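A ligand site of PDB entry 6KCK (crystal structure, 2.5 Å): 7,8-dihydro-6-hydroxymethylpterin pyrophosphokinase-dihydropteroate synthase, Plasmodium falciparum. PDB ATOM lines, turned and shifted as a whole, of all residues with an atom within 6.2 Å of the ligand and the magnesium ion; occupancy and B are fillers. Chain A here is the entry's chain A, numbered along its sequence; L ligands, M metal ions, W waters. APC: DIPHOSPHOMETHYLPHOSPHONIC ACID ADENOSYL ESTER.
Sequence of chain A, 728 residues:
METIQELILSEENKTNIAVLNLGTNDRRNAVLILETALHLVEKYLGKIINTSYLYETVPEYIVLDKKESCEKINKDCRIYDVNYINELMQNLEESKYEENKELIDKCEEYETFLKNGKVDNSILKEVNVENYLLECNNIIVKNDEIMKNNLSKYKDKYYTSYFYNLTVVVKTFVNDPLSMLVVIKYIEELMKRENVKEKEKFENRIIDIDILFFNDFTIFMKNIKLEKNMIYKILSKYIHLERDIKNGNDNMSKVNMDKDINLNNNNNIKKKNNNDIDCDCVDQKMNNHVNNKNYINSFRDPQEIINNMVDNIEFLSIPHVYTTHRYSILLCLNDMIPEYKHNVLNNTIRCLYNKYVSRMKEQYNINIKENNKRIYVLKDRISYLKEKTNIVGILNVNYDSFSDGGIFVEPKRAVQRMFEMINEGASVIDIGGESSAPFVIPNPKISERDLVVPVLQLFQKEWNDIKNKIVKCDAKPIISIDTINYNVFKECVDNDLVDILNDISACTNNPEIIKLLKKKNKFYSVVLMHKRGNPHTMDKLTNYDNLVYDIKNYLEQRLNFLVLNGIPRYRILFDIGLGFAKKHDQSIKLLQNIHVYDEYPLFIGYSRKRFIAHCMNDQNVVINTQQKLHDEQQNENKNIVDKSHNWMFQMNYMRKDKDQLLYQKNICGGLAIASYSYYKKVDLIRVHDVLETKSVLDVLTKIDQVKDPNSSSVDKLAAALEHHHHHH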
ATOM      1  N   ASN A 143      14.952   6.955  -4.477  1.00  0.00           N
ATOM      2  CA  ASN A 143      14.818   6.650  -3.051  1.00  0.00           C
ATOM      3  C   ASN A 143      16.080   6.032  -2.442  1.00  0.00           C
ATOM      4  O   ASN A 143      16.265   6.064  -1.223  1.00  0.00           O
ATOM      5  CB  ASN A 143      13.604   5.745  -2.797  1.00  0.00           C
ATOM      6  CG  ASN A 143      12.270   6.475  -2.933  1.00  0.00           C
ATOM      7  OD1 ASN A 143      12.174   7.688  -2.712  1.00  0.00           O
ATOM      8  ND2 ASN A 143      11.233   5.735  -3.295  1.00  0.00           N
ATOM      9  N   LEU A 181      -7.554   4.401  -4.040  1.00  0.00           N
ATOM     10  CA  LEU A 181      -6.497   5.108  -3.343  1.00  0.00           C
ATOM     11  C   LEU A 181      -7.039   6.357  -2.642  1.00  0.00           C
ATOM     12  O   LEU A 181      -6.548   6.748  -1.571  1.00  0.00           O
ATOM     13  CB  LEU A 181      -5.328   5.435  -4.270  1.00  0.00           C
ATOM     14  CG  LEU A 181      -4.080   6.036  -3.581  1.00  0.00           C
ATOM     15  CD1 LEU A 181      -3.560   5.116  -2.478  1.00  0.00           C
ATOM     16  CD2 LEU A 181      -2.959   6.360  -4.556  1.00  0.00           C
ATOM     17  N   LYS A 185      -7.019   6.888   1.304  1.00  0.00           N
ATOM     18  CA  LYS A 185      -6.444   8.075   1.949  1.00  0.00           C
ATOM     19  C   LYS A 185      -7.381   8.704   2.979  1.00  0.00           C
ATOM     20  O   LYS A 185      -6.946   9.194   4.020  1.00  0.00           O
ATOM     21  CB  LYS A 185      -6.004   9.126   0.927  1.00  0.00           C
ATOM     22  CG  LYS A 185      -4.794   8.732   0.110  1.00  0.00           C
ATOM     23  CD  LYS A 185      -3.614   8.351   0.987  1.00  0.00           C
ATOM     24  CE  LYS A 185      -2.397   7.998   0.151  1.00  0.00           C
ATOM     25  NZ  LYS A 185      -1.353   7.383   1.013  1.00  0.00           N
ATOM     26  N   GLU A 188      -6.906   6.701   6.109  1.00  0.00           N
ATOM     27  CA  GLU A 188      -5.671   7.046   6.815  1.00  0.00           C
ATOM     28  C   GLU A 188      -5.850   8.346   7.621  1.00  0.00           C
ATOM     29  O   GLU A 188      -5.450   8.419   8.788  1.00  0.00           O
ATOM     30  CB  GLU A 188      -4.457   7.136   5.883  1.00  0.00           C
ATOM     31  CG  GLU A 188      -4.122   5.843   5.152  1.00  0.00           C
ATOM     32  CD  GLU A 188      -2.873   5.936   4.306  1.00  0.00           C
ATOM     33  OE1 GLU A 188      -2.478   7.030   3.882  1.00  0.00           O
ATOM     34  OE2 GLU A 188      -2.246   4.889   4.037  1.00  0.00           O
ATOM     35  N   ARG A 205       4.105   6.869   9.820  1.00  0.00           N
ATOM     36  CA  ARG A 205       3.210   7.433  10.832  1.00  0.00           C
ATOM     37  C   ARG A 205       2.375   6.351  11.547  1.00  0.00           C
ATOM     38  O   ARG A 205       2.907   5.276  11.880  1.00  0.00           O
ATOM     39  CB  ARG A 205       2.338   8.574  10.252  1.00  0.00           C
ATOM     40  CG  ARG A 205       1.420   8.191   9.096  1.00  0.00           C
ATOM     41  CD  ARG A 205       2.053   8.375   7.717  1.00  0.00           C
ATOM     42  NE  ARG A 205       1.158   7.911   6.643  1.00  0.00           N
ATOM     43  CZ  ARG A 205       1.577   7.432   5.476  1.00  0.00           C
ATOM     44  NH1 ARG A 205       2.874   7.321   5.218  1.00  0.00           N
ATOM     45  NH2 ARG A 205       0.687   7.031   4.562  1.00  0.00           N
ATOM     46  N   ASP A 208      -0.153   2.983   7.309  1.00  0.00           N
ATOM     47  CA  ASP A 208       0.165   3.100   5.884  1.00  0.00           C
ATOM     48  C   ASP A 208      -0.579   2.004   5.137  1.00  0.00           C
ATOM     49  O   ASP A 208      -0.416   0.821   5.448  1.00  0.00           O
ATOM     50  CB  ASP A 208       1.690   2.963   5.611  1.00  0.00           C
ATOM     51  CG  ASP A 208       2.063   3.210   4.131  1.00  0.00           C
ATOM     52  OD1 ASP A 208       1.200   3.600   3.332  1.00  0.00           O
ATOM     53  OD2 ASP A 208       3.225   3.000   3.731  1.00  0.00           O
ATOM     54  N   ILE A 209      -1.387   2.382   4.157  1.00  0.00           N
ATOM     55  CA  ILE A 209      -2.192   1.407   3.410  1.00  0.00           C
ATOM     56  C   ILE A 209      -1.861   1.543   1.937  1.00  0.00           C
ATOM     57  O   ILE A 209      -2.211   2.543   1.317  1.00  0.00           O
ATOM     58  CB  ILE A 209      -3.719   1.571   3.641  1.00  0.00           C
ATOM     59  CG1 ILE A 209      -4.051   1.507   5.134  1.00  0.00           C
ATOM     60  CG2 ILE A 209      -4.524   0.503   2.894  1.00  0.00           C
ATOM     61  CD1 ILE A 209      -5.522   1.710   5.458  1.00  0.00           C
ATOM     62  N   ASP A 210      -1.189   0.536   1.388  1.00  0.00           N
ATOM     63  CA  ASP A 210      -0.796   0.508   0.000  1.00  0.00           C
ATOM     64  C   ASP A 210      -1.651  -0.444  -0.838  1.00  0.00           C
ATOM     65  O   ASP A 210      -2.179  -1.426  -0.324  1.00  0.00           O
ATOM     66  CB  ASP A 210       0.670   0.084  -0.104  1.00  0.00           C
ATOM     67  CG  ASP A 210       1.595   1.024   0.664  1.00  0.00           C
ATOM     68  OD1 ASP A 210       1.388   2.257   0.602  1.00  0.00           O
ATOM     69  OD2 ASP A 210       2.531   0.517   1.329  1.00  0.00           O
ATOM     70  N   ILE A 211      -1.789  -0.155  -2.126  1.00  0.00           N
ATOM     71  CA  ILE A 211      -2.447  -1.089  -3.011  1.00  0.00           C
ATOM     72  C   ILE A 211      -1.357  -1.896  -3.680  1.00  0.00           C
ATOM     73  O   ILE A 211      -0.572  -1.339  -4.434  1.00  0.00           O
ATOM     74  CB  ILE A 211      -3.299  -0.410  -4.092  1.00  0.00           C
ATOM     75  CG1 ILE A 211      -4.247   0.619  -3.448  1.00  0.00           C
ATOM     76  CG2 ILE A 211      -4.063  -1.473  -4.899  1.00  0.00           C
ATOM     77  CD1 ILE A 211      -5.235   1.248  -4.417  1.00  0.00           C
ATOM     78  N   LEU A 212      -1.284  -3.190  -3.379  1.00  0.00           N
ATOM     79  CA  LEU A 212      -0.301  -4.039  -4.053  1.00  0.00           C
ATOM     80  C   LEU A 212      -0.819  -4.427  -5.420  1.00  0.00           C
ATOM     81  O   LEU A 212      -0.147  -4.206  -6.404  1.00  0.00           O
ATOM     82  CB  LEU A 212       0.084  -5.263  -3.231  1.00  0.00           C
ATOM     83  CG  LEU A 212       0.561  -4.959  -1.783  1.00  0.00           C
ATOM     84  CD1 LEU A 212       0.702  -6.255  -0.993  1.00  0.00           C
ATOM     85  CD2 LEU A 212       1.860  -4.137  -1.733  1.00  0.00           C
ATOM     86  N   ASP A 311      -2.464  16.867  -1.990  1.00  0.00           N
ATOM     87  CA  ASP A 311      -1.037  16.769  -2.287  1.00  0.00           C
ATOM     88  C   ASP A 311      -0.527  15.345  -2.067  1.00  0.00           C
ATOM     89  O   ASP A 311       0.593  15.012  -2.481  1.00  0.00           O
ATOM     90  CB  ASP A 311      -0.241  17.771  -1.438  1.00  0.00           C
ATOM     91  CG  ASP A 311      -0.527  19.220  -1.823  1.00  0.00           C
ATOM     92  OD1 ASP A 311      -0.320  19.587  -3.001  1.00  0.00           O
ATOM     93  OD2 ASP A 311      -0.959  19.993  -0.936  1.00  0.00           O
ATOM     94  N   ASN A 312      -1.337  14.508  -1.428  1.00  0.00           N
ATOM     95  CA  ASN A 312      -0.924  13.157  -1.040  1.00  0.00           C
ATOM     96  C   ASN A 312      -0.885  12.141  -2.192  1.00  0.00           C
ATOM     97  O   ASN A 312       0.002  11.296  -2.253  1.00  0.00           O
ATOM     98  CB  ASN A 312      -1.738  12.635   0.148  1.00  0.00           C
ATOM     99  CG  ASN A 312      -1.314  13.247   1.482  1.00  0.00           C
ATOM    100  OD1 ASN A 312      -0.221  13.798   1.619  1.00  0.00           O
ATOM    101  ND2 ASN A 312      -2.180  13.141   2.482  1.00  0.00           N
ATOM    102  N   ILE A 313      -1.834  12.249  -3.116  1.00  0.00           N
ATOM    103  CA  ILE A 313      -1.831  11.378  -4.290  1.00  0.00           C
ATOM    104  C   ILE A 313      -0.982  12.039  -5.360  1.00  0.00           C
ATOM    105  O   ILE A 313      -1.391  13.016  -5.979  1.00  0.00           O
ATOM    106  CB  ILE A 313      -3.254  11.091  -4.807  1.00  0.00           C
ATOM    107  CG1 ILE A 313      -4.108  10.452  -3.707  1.00  0.00           C
ATOM    108  CG2 ILE A 313      -3.223  10.180  -6.035  1.00  0.00           C
ATOM    109  CD1 ILE A 313      -5.591  10.465  -4.001  1.00  0.00           C
ATOM    110  N   GLU A 314       0.220  11.493  -5.556  1.00  0.00           N
ATOM    111  CA  GLU A 314       1.199  12.068  -6.474  1.00  0.00           C
ATOM    112  C   GLU A 314       1.215  11.263  -7.761  1.00  0.00           C
ATOM    113  O   GLU A 314       1.135  11.813  -8.858  1.00  0.00           O
ATOM    114  CB  GLU A 314       2.599  12.083  -5.838  1.00  0.00           C
ATOM    115  CG  GLU A 314       3.719  12.554  -6.750  1.00  0.00           C
ATOM    116  CD  GLU A 314       5.076  11.912  -6.458  1.00  0.00           C
ATOM    117  OE1 GLU A 314       5.232  11.273  -5.397  1.00  0.00           O
ATOM    118  OE2 GLU A 314       6.004  12.041  -7.309  1.00  0.00           O
ATOM    119  N   PHE A 315       1.321   9.955  -7.608  1.00  0.00           N
ATOM    120  CA  PHE A 315       1.306   9.023  -8.724  1.00  0.00           C
ATOM    121  C   PHE A 315       0.619   7.736  -8.297  1.00  0.00           C
ATOM    122  O   PHE A 315       0.301   7.581  -7.126  1.00  0.00           O
ATOM    123  CB  PHE A 315       2.734   8.788  -9.244  1.00  0.00           C
ATOM    124  CG  PHE A 315       3.569   7.928  -8.338  1.00  0.00           C
ATOM    125  CD1 PHE A 315       4.132   8.434  -7.178  1.00  0.00           C
ATOM    126  CD2 PHE A 315       3.809   6.583  -8.668  1.00  0.00           C
ATOM    127  CE1 PHE A 315       4.907   7.638  -6.358  1.00  0.00           C
ATOM    128  CE2 PHE A 315       4.596   5.789  -7.853  1.00  0.00           C
ATOM    129  CZ  PHE A 315       5.137   6.310  -6.701  1.00  0.00           C
ATOM    130  N   LEU A 316       0.375   6.831  -9.240  1.00  0.00           N
ATOM    131  CA  LEU A 316      -0.203   5.516  -8.954  1.00  0.00           C
ATOM    132  C   LEU A 316       0.475   4.392  -9.724  1.00  0.00           C
ATOM    133  O   LEU A 316       0.416   4.343 -10.951  1.00  0.00           O
ATOM    134  CB  LEU A 316      -1.710   5.507  -9.193  1.00  0.00           C
ATOM    135  CG  LEU A 316      -2.466   4.194  -8.927  1.00  0.00           C
ATOM    136  CD1 LEU A 316      -2.595   3.896  -7.426  1.00  0.00           C
ATOM    137  CD2 LEU A 316      -3.836   4.225  -9.585  1.00  0.00           C
ATOM    138  N   SER A 317       1.097   3.478  -8.977  1.00  0.00           N
ATOM    139  CA  SER A 317       1.735   2.310  -9.539  1.00  0.00           C
ATOM    140  C   SER A 317       1.012   1.036  -9.113  1.00  0.00           C
ATOM    141  O   SER A 317       0.907   0.772  -7.921  1.00  0.00           O
ATOM    142  CB  SER A 317       3.187   2.233  -9.054  1.00  0.00           C
ATOM    143  OG  SER A 317       3.846   1.137  -9.661  1.00  0.00           O
ATOM    144  N   ILE A 318       0.519   0.262 -10.079  1.00  0.00           N
ATOM    145  CA  ILE A 318      -0.022  -1.071  -9.855  1.00  0.00           C
ATOM    146  C   ILE A 318       0.724  -2.055 -10.728  1.00  0.00           C
ATOM    147  O   ILE A 318       0.660  -1.950 -11.947  1.00  0.00           O
ATOM    148  CB  ILE A 318      -1.522  -1.210 -10.218  1.00  0.00           C
ATOM    149  CG1 ILE A 318      -2.422  -0.262  -9.410  1.00  0.00           C
ATOM    150  CG2 ILE A 318      -1.985  -2.654 -10.052  1.00  0.00           C
ATOM    151  CD1 ILE A 318      -2.199  -0.233  -7.924  1.00  0.00           C
ATOM    152  N   PRO A 319       1.416  -3.037 -10.137  1.00  0.00           N
ATOM    153  CA  PRO A 319       1.717  -3.306  -8.740  1.00  0.00           C
ATOM    154  C   PRO A 319       2.447  -2.167  -8.073  1.00  0.00           C
ATOM    155  O   PRO A 319       3.085  -1.369  -8.750  1.00  0.00           O
ATOM    156  CB  PRO A 319       2.696  -4.484  -8.844  1.00  0.00           C
ATOM    157  CG  PRO A 319       2.183  -5.235 -10.018  1.00  0.00           C
ATOM    158  CD  PRO A 319       1.859  -4.143 -10.989  1.00  0.00           C
ATOM    159  N   HIS A 320       2.342  -2.105  -6.754  1.00  0.00           N
ATOM    160  CA  HIS A 320       3.080  -1.150  -5.957  1.00  0.00           C
ATOM    161  C   HIS A 320       4.537  -1.333  -6.254  1.00  0.00           C
ATOM    162  O   HIS A 320       4.997  -2.453  -6.495  1.00  0.00           O
ATOM    163  CB  HIS A 320       2.821  -1.446  -4.490  1.00  0.00           C
ATOM    164  CG  HIS A 320       3.309  -0.378  -3.547  1.00  0.00           C
ATOM    165  ND1 HIS A 320       4.579  -0.304  -3.136  1.00  0.00           N
ATOM    166  CD2 HIS A 320       2.635   0.664  -2.924  1.00  0.00           C
ATOM    167  CE1 HIS A 320       4.723   0.727  -2.302  1.00  0.00           C
ATOM    168  NE2 HIS A 320       3.526   1.319  -2.179  1.00  0.00           N
ATOM    169  N   VAL A 321       5.288  -0.244  -6.204  1.00  0.00           N
ATOM    170  CA  VAL A 321       6.712  -0.266  -6.576  1.00  0.00           C
ATOM    171  C   VAL A 321       7.522  -1.281  -5.774  1.00  0.00           C
ATOM    172  O   VAL A 321       8.301  -2.052  -6.350  1.00  0.00           O
ATOM    173  CB  VAL A 321       7.322   1.147  -6.458  1.00  0.00           C
ATOM    174  CG1 VAL A 321       8.834   1.113  -6.546  1.00  0.00           C
ATOM    175  CG2 VAL A 321       6.773   2.031  -7.550  1.00  0.00           C
ATOM    176  N   TYR A 322       7.317  -1.300  -4.459  1.00  0.00           N
ATOM    177  CA  TYR A 322       8.129  -2.156  -3.582  1.00  0.00           C
ATOM    178  C   TYR A 322       7.696  -3.623  -3.394  1.00  0.00           C
ATOM    179  O   TYR A 322       8.301  -4.374  -2.612  1.00  0.00           O
ATOM    180  CB  TYR A 322       8.329  -1.457  -2.253  1.00  0.00           C
ATOM    181  CG  TYR A 322       9.286  -0.298  -2.374  1.00  0.00           C
ATOM    182  CD1 TYR A 322      10.664  -0.530  -2.413  1.00  0.00           C
ATOM    183  CD2 TYR A 322       8.815   1.010  -2.475  1.00  0.00           C
ATOM    184  CE1 TYR A 322      11.559   0.525  -2.535  1.00  0.00           C
ATOM    185  CE2 TYR A 322       9.698   2.073  -2.601  1.00  0.00           C
ATOM    186  CZ  TYR A 322      11.064   1.819  -2.623  1.00  0.00           C
ATOM    187  OH  TYR A 322      11.960   2.854  -2.734  1.00  0.00           O
ATOM    188  N   ARG A 326      10.565  -5.617  -1.293  1.00  0.00           N
ATOM    189  CA  ARG A 326      10.477  -5.521   0.169  1.00  0.00           C
ATOM    190  C   ARG A 326      10.147  -6.888   0.743  1.00  0.00           C
ATOM    191  O   ARG A 326       9.094  -7.443   0.429  1.00  0.00           O
ATOM    192  CB  ARG A 326       9.423  -4.503   0.533  1.00  0.00           C
ATOM    193  CG  ARG A 326       9.816  -3.575   1.655  1.00  0.00           C
ATOM    194  CD  ARG A 326       8.948  -2.333   1.617  1.00  0.00           C
ATOM    195  NE  ARG A 326       9.763  -1.129   1.530  1.00  0.00           N
ATOM    196  CZ  ARG A 326       9.302   0.073   1.190  1.00  0.00           C
ATOM    197  NH1 ARG A 326       8.015   0.249   0.910  1.00  0.00           N
ATOM    198  NH2 ARG A 326      10.144   1.101   1.144  1.00  0.00           N
HETATM  199  PG  APC L   1       6.212   3.491   0.187  1.00  0.00           P
HETATM  200  O1G APC L   1       5.124   2.816   1.015  1.00  0.00           O
HETATM  201  O2G APC L   1       5.700   4.339  -0.956  1.00  0.00           O
HETATM  202  O3G APC L   1       7.337   2.567  -0.226  1.00  0.00           O
HETATM  203  PB  APC L   1       6.125   5.632   2.041  1.00  0.00           P
HETATM  204  O1B APC L   1       5.223   4.974   3.008  1.00  0.00           O
HETATM  205  O2B APC L   1       7.176   6.539   2.842  1.00  0.00           O
HETATM  206  O3B APC L   1       6.934   4.530   1.190  1.00  0.00           O
HETATM  207  PA  APC L   1       3.432   6.772   1.367  1.00  0.00           P
HETATM  208  O1A APC L   1       2.786   5.445   1.545  1.00  0.00           O
HETATM  209  O2A APC L   1       3.293   7.609   2.738  1.00  0.00           O
HETATM  210  C3A APC L   1       5.173   6.655   0.894  1.00  0.00           C
HETATM  211  O5' APC L   1       2.707   7.572   0.183  1.00  0.00           O
HETATM  212  C5' APC L   1       2.212   6.859  -0.943  1.00  0.00           C
HETATM  213  C4' APC L   1       2.007   7.787  -2.116  1.00  0.00           C
HETATM  214  O4' APC L   1       2.689   7.222  -3.234  1.00  0.00           O
HETATM  215  C3' APC L   1       0.538   7.817  -2.490  1.00  0.00           C
HETATM  216  O3' APC L   1      -0.155   8.924  -1.916  1.00  0.00           O
HETATM  217  C2' APC L   1       0.580   7.955  -3.979  1.00  0.00           C
HETATM  218  O2' APC L   1       0.849   9.328  -4.288  1.00  0.00           O
HETATM  219  C1' APC L   1       1.809   7.156  -4.366  1.00  0.00           C
HETATM  220  N9  APC L   1       1.443   5.761  -4.790  1.00  0.00           N
HETATM  221  C8  APC L   1       1.713   5.259  -6.009  1.00  0.00           C
HETATM  222  N7  APC L   1       1.288   3.984  -6.158  1.00  0.00           N
HETATM  223  C5  APC L   1       0.716   3.633  -5.001  1.00  0.00           C
HETATM  224  C6  APC L   1       0.048   2.419  -4.461  1.00  0.00           C
HETATM  225  N6  APC L   1      -0.081   1.295  -5.215  1.00  0.00           N
HETATM  226  N1  APC L   1      -0.425   2.463  -3.196  1.00  0.00           N
HETATM  227  C2  APC L   1      -0.299   3.558  -2.411  1.00  0.00           C
HETATM  228  N3  APC L   1       0.296   4.683  -2.839  1.00  0.00           N
HETATM  229  C4  APC L   1       0.815   4.802  -4.098  1.00  0.00           C
HETATM  230 MG    MG M   1       2.911   3.548   1.567  1.00  0.00          MG
HETATM  231  O   HOH W   1       3.896   2.394  -5.100  1.00  0.00           O
HETATM  232  O   HOH W   2      -0.121   4.590   1.061  1.00  0.00           O
HETATM  233  O   HOH W   3       5.703   3.161   4.754  1.00  0.00           O
HETATM  234  O   HOH W   4       4.146   4.755  -2.990  1.00  0.00           O
HETATM  235  O   HOH W   5       2.839   3.817  -0.767  1.00  0.00           O
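Water W5 lies within hydrogen-bond range of O2G of the ligand (2.9 Å) and NE2 of His 320 (3.0 Å).
Water W2 bridges the backbone carbonyl oxygen (O) of Ile 209 and the side-chain amino group (NZ) of Lys 185.
Water W1 lies within hydrogen-bond range of NE2 of His 320 (3.1 Å), N of Val 321 (3.2 Å) and N7 of the ligand (3.2 Å).
Leu 181 touches the ligand.
Lys 185 touches the ligand (CE to O3', 3.2 Å).
Ile 313 touches the ligand (CA to O2', 3.4 Å).
Leu 316 touches the ligand (CA to N7, 3.5 Å).
Ile 318 touches the ligand.
His 320 touches the ligand.
Tyr 322 touches the ligand.
Hydrophobic or aromatic side chains that line the ligand: Leu 181, Ile 211, Phe 315, Ile 318, His 320 and Tyr 322.
Of the 23 residues printed, 16 come within 4 Å of the ligand.
The nearest printed residue that does not touch the ligand is Ile 209 (4.3 Å).
The backbone NH of His 320 sits at hydrogen-bond distance from the backbone carbonyl oxygen of Leu 212 (3.3 Å).
The side-chain hydroxyl (OH) of Tyr 322 sits at hydrogen-bond distance from the side-chain amide nitrogen (ND2) of Asn 143.
The side-chain amino group of Lys 185 lies within salt-bridge range of the side-chain carboxylate of Glu 188, 3.1 Å away.
The side-chain carboxylate of Asp 208 lies close to the guanidinium group of Arg 205 (3.7 Å).
OG of Ser 317 is in hydrogen-bond range of O of Pro 319 (2.8 Å).
The backbone NH (N) of Tyr 322 lies within hydrogen-bond range of a ring nitrogen (ND1) of His 320.
The side-chain carboxylate of Glu 188 lies within salt-bridge range of the guanidinium group of Arg 205.
The backbone NH (N) of Ile 211 sits at hydrogen-bond distance from a nitrogen (N1) of the ligand, at 3.1 Å.
NH1 of Arg 326 lies within salt-bridge range of O3G of the ligand, at 2.7 Å.
A nitrogen (N6) of the ligand sits at hydrogen-bond distance from the backbone carbonyl oxygen (O) of Ile 211, at 2.8 Å.
The backbone NH of Glu 314 is in hydrogen-bond range of an oxygen (O2') of the ligand, 2.6 Å away.
A nitrogen (N6) of the ligand sits at hydrogen-bond distance from the backbone carbonyl oxygen of Ser 317, at 2.9 Å.
An oxygen (O2') of the ligand lies close to the backbone carbonyl oxygen (O) of Phe 315 (3.4 Å).
The guanidinium group (NH1) of Arg 205 is in salt-bridge range of an oxygen (O2A) of the ligand (2.5 Å).
N of Ser 317 is in hydrogen-bond range of N7 of the ligand.
O of Asn 312 is in hydrogen-bond range of O3' of the ligand (2.4 Å).
The backbone NH (N) of Phe 315 is in hydrogen-bond range of an oxygen (O2') of the ligand.
O1A of the ligand binds the magnesium ion.
OD1 of Asp 210 binds the magnesium ion (2.2 Å).
OD2 of Asp 208 is bound to the magnesium ion (2.3 Å).
Water W5 is bound to the magnesium ion (2.4 Å).
O1G of the ligand binds the magnesium ion.
The side-chain carboxylate (OD1) of Asp 208 binds the magnesium ion (2.5 Å).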
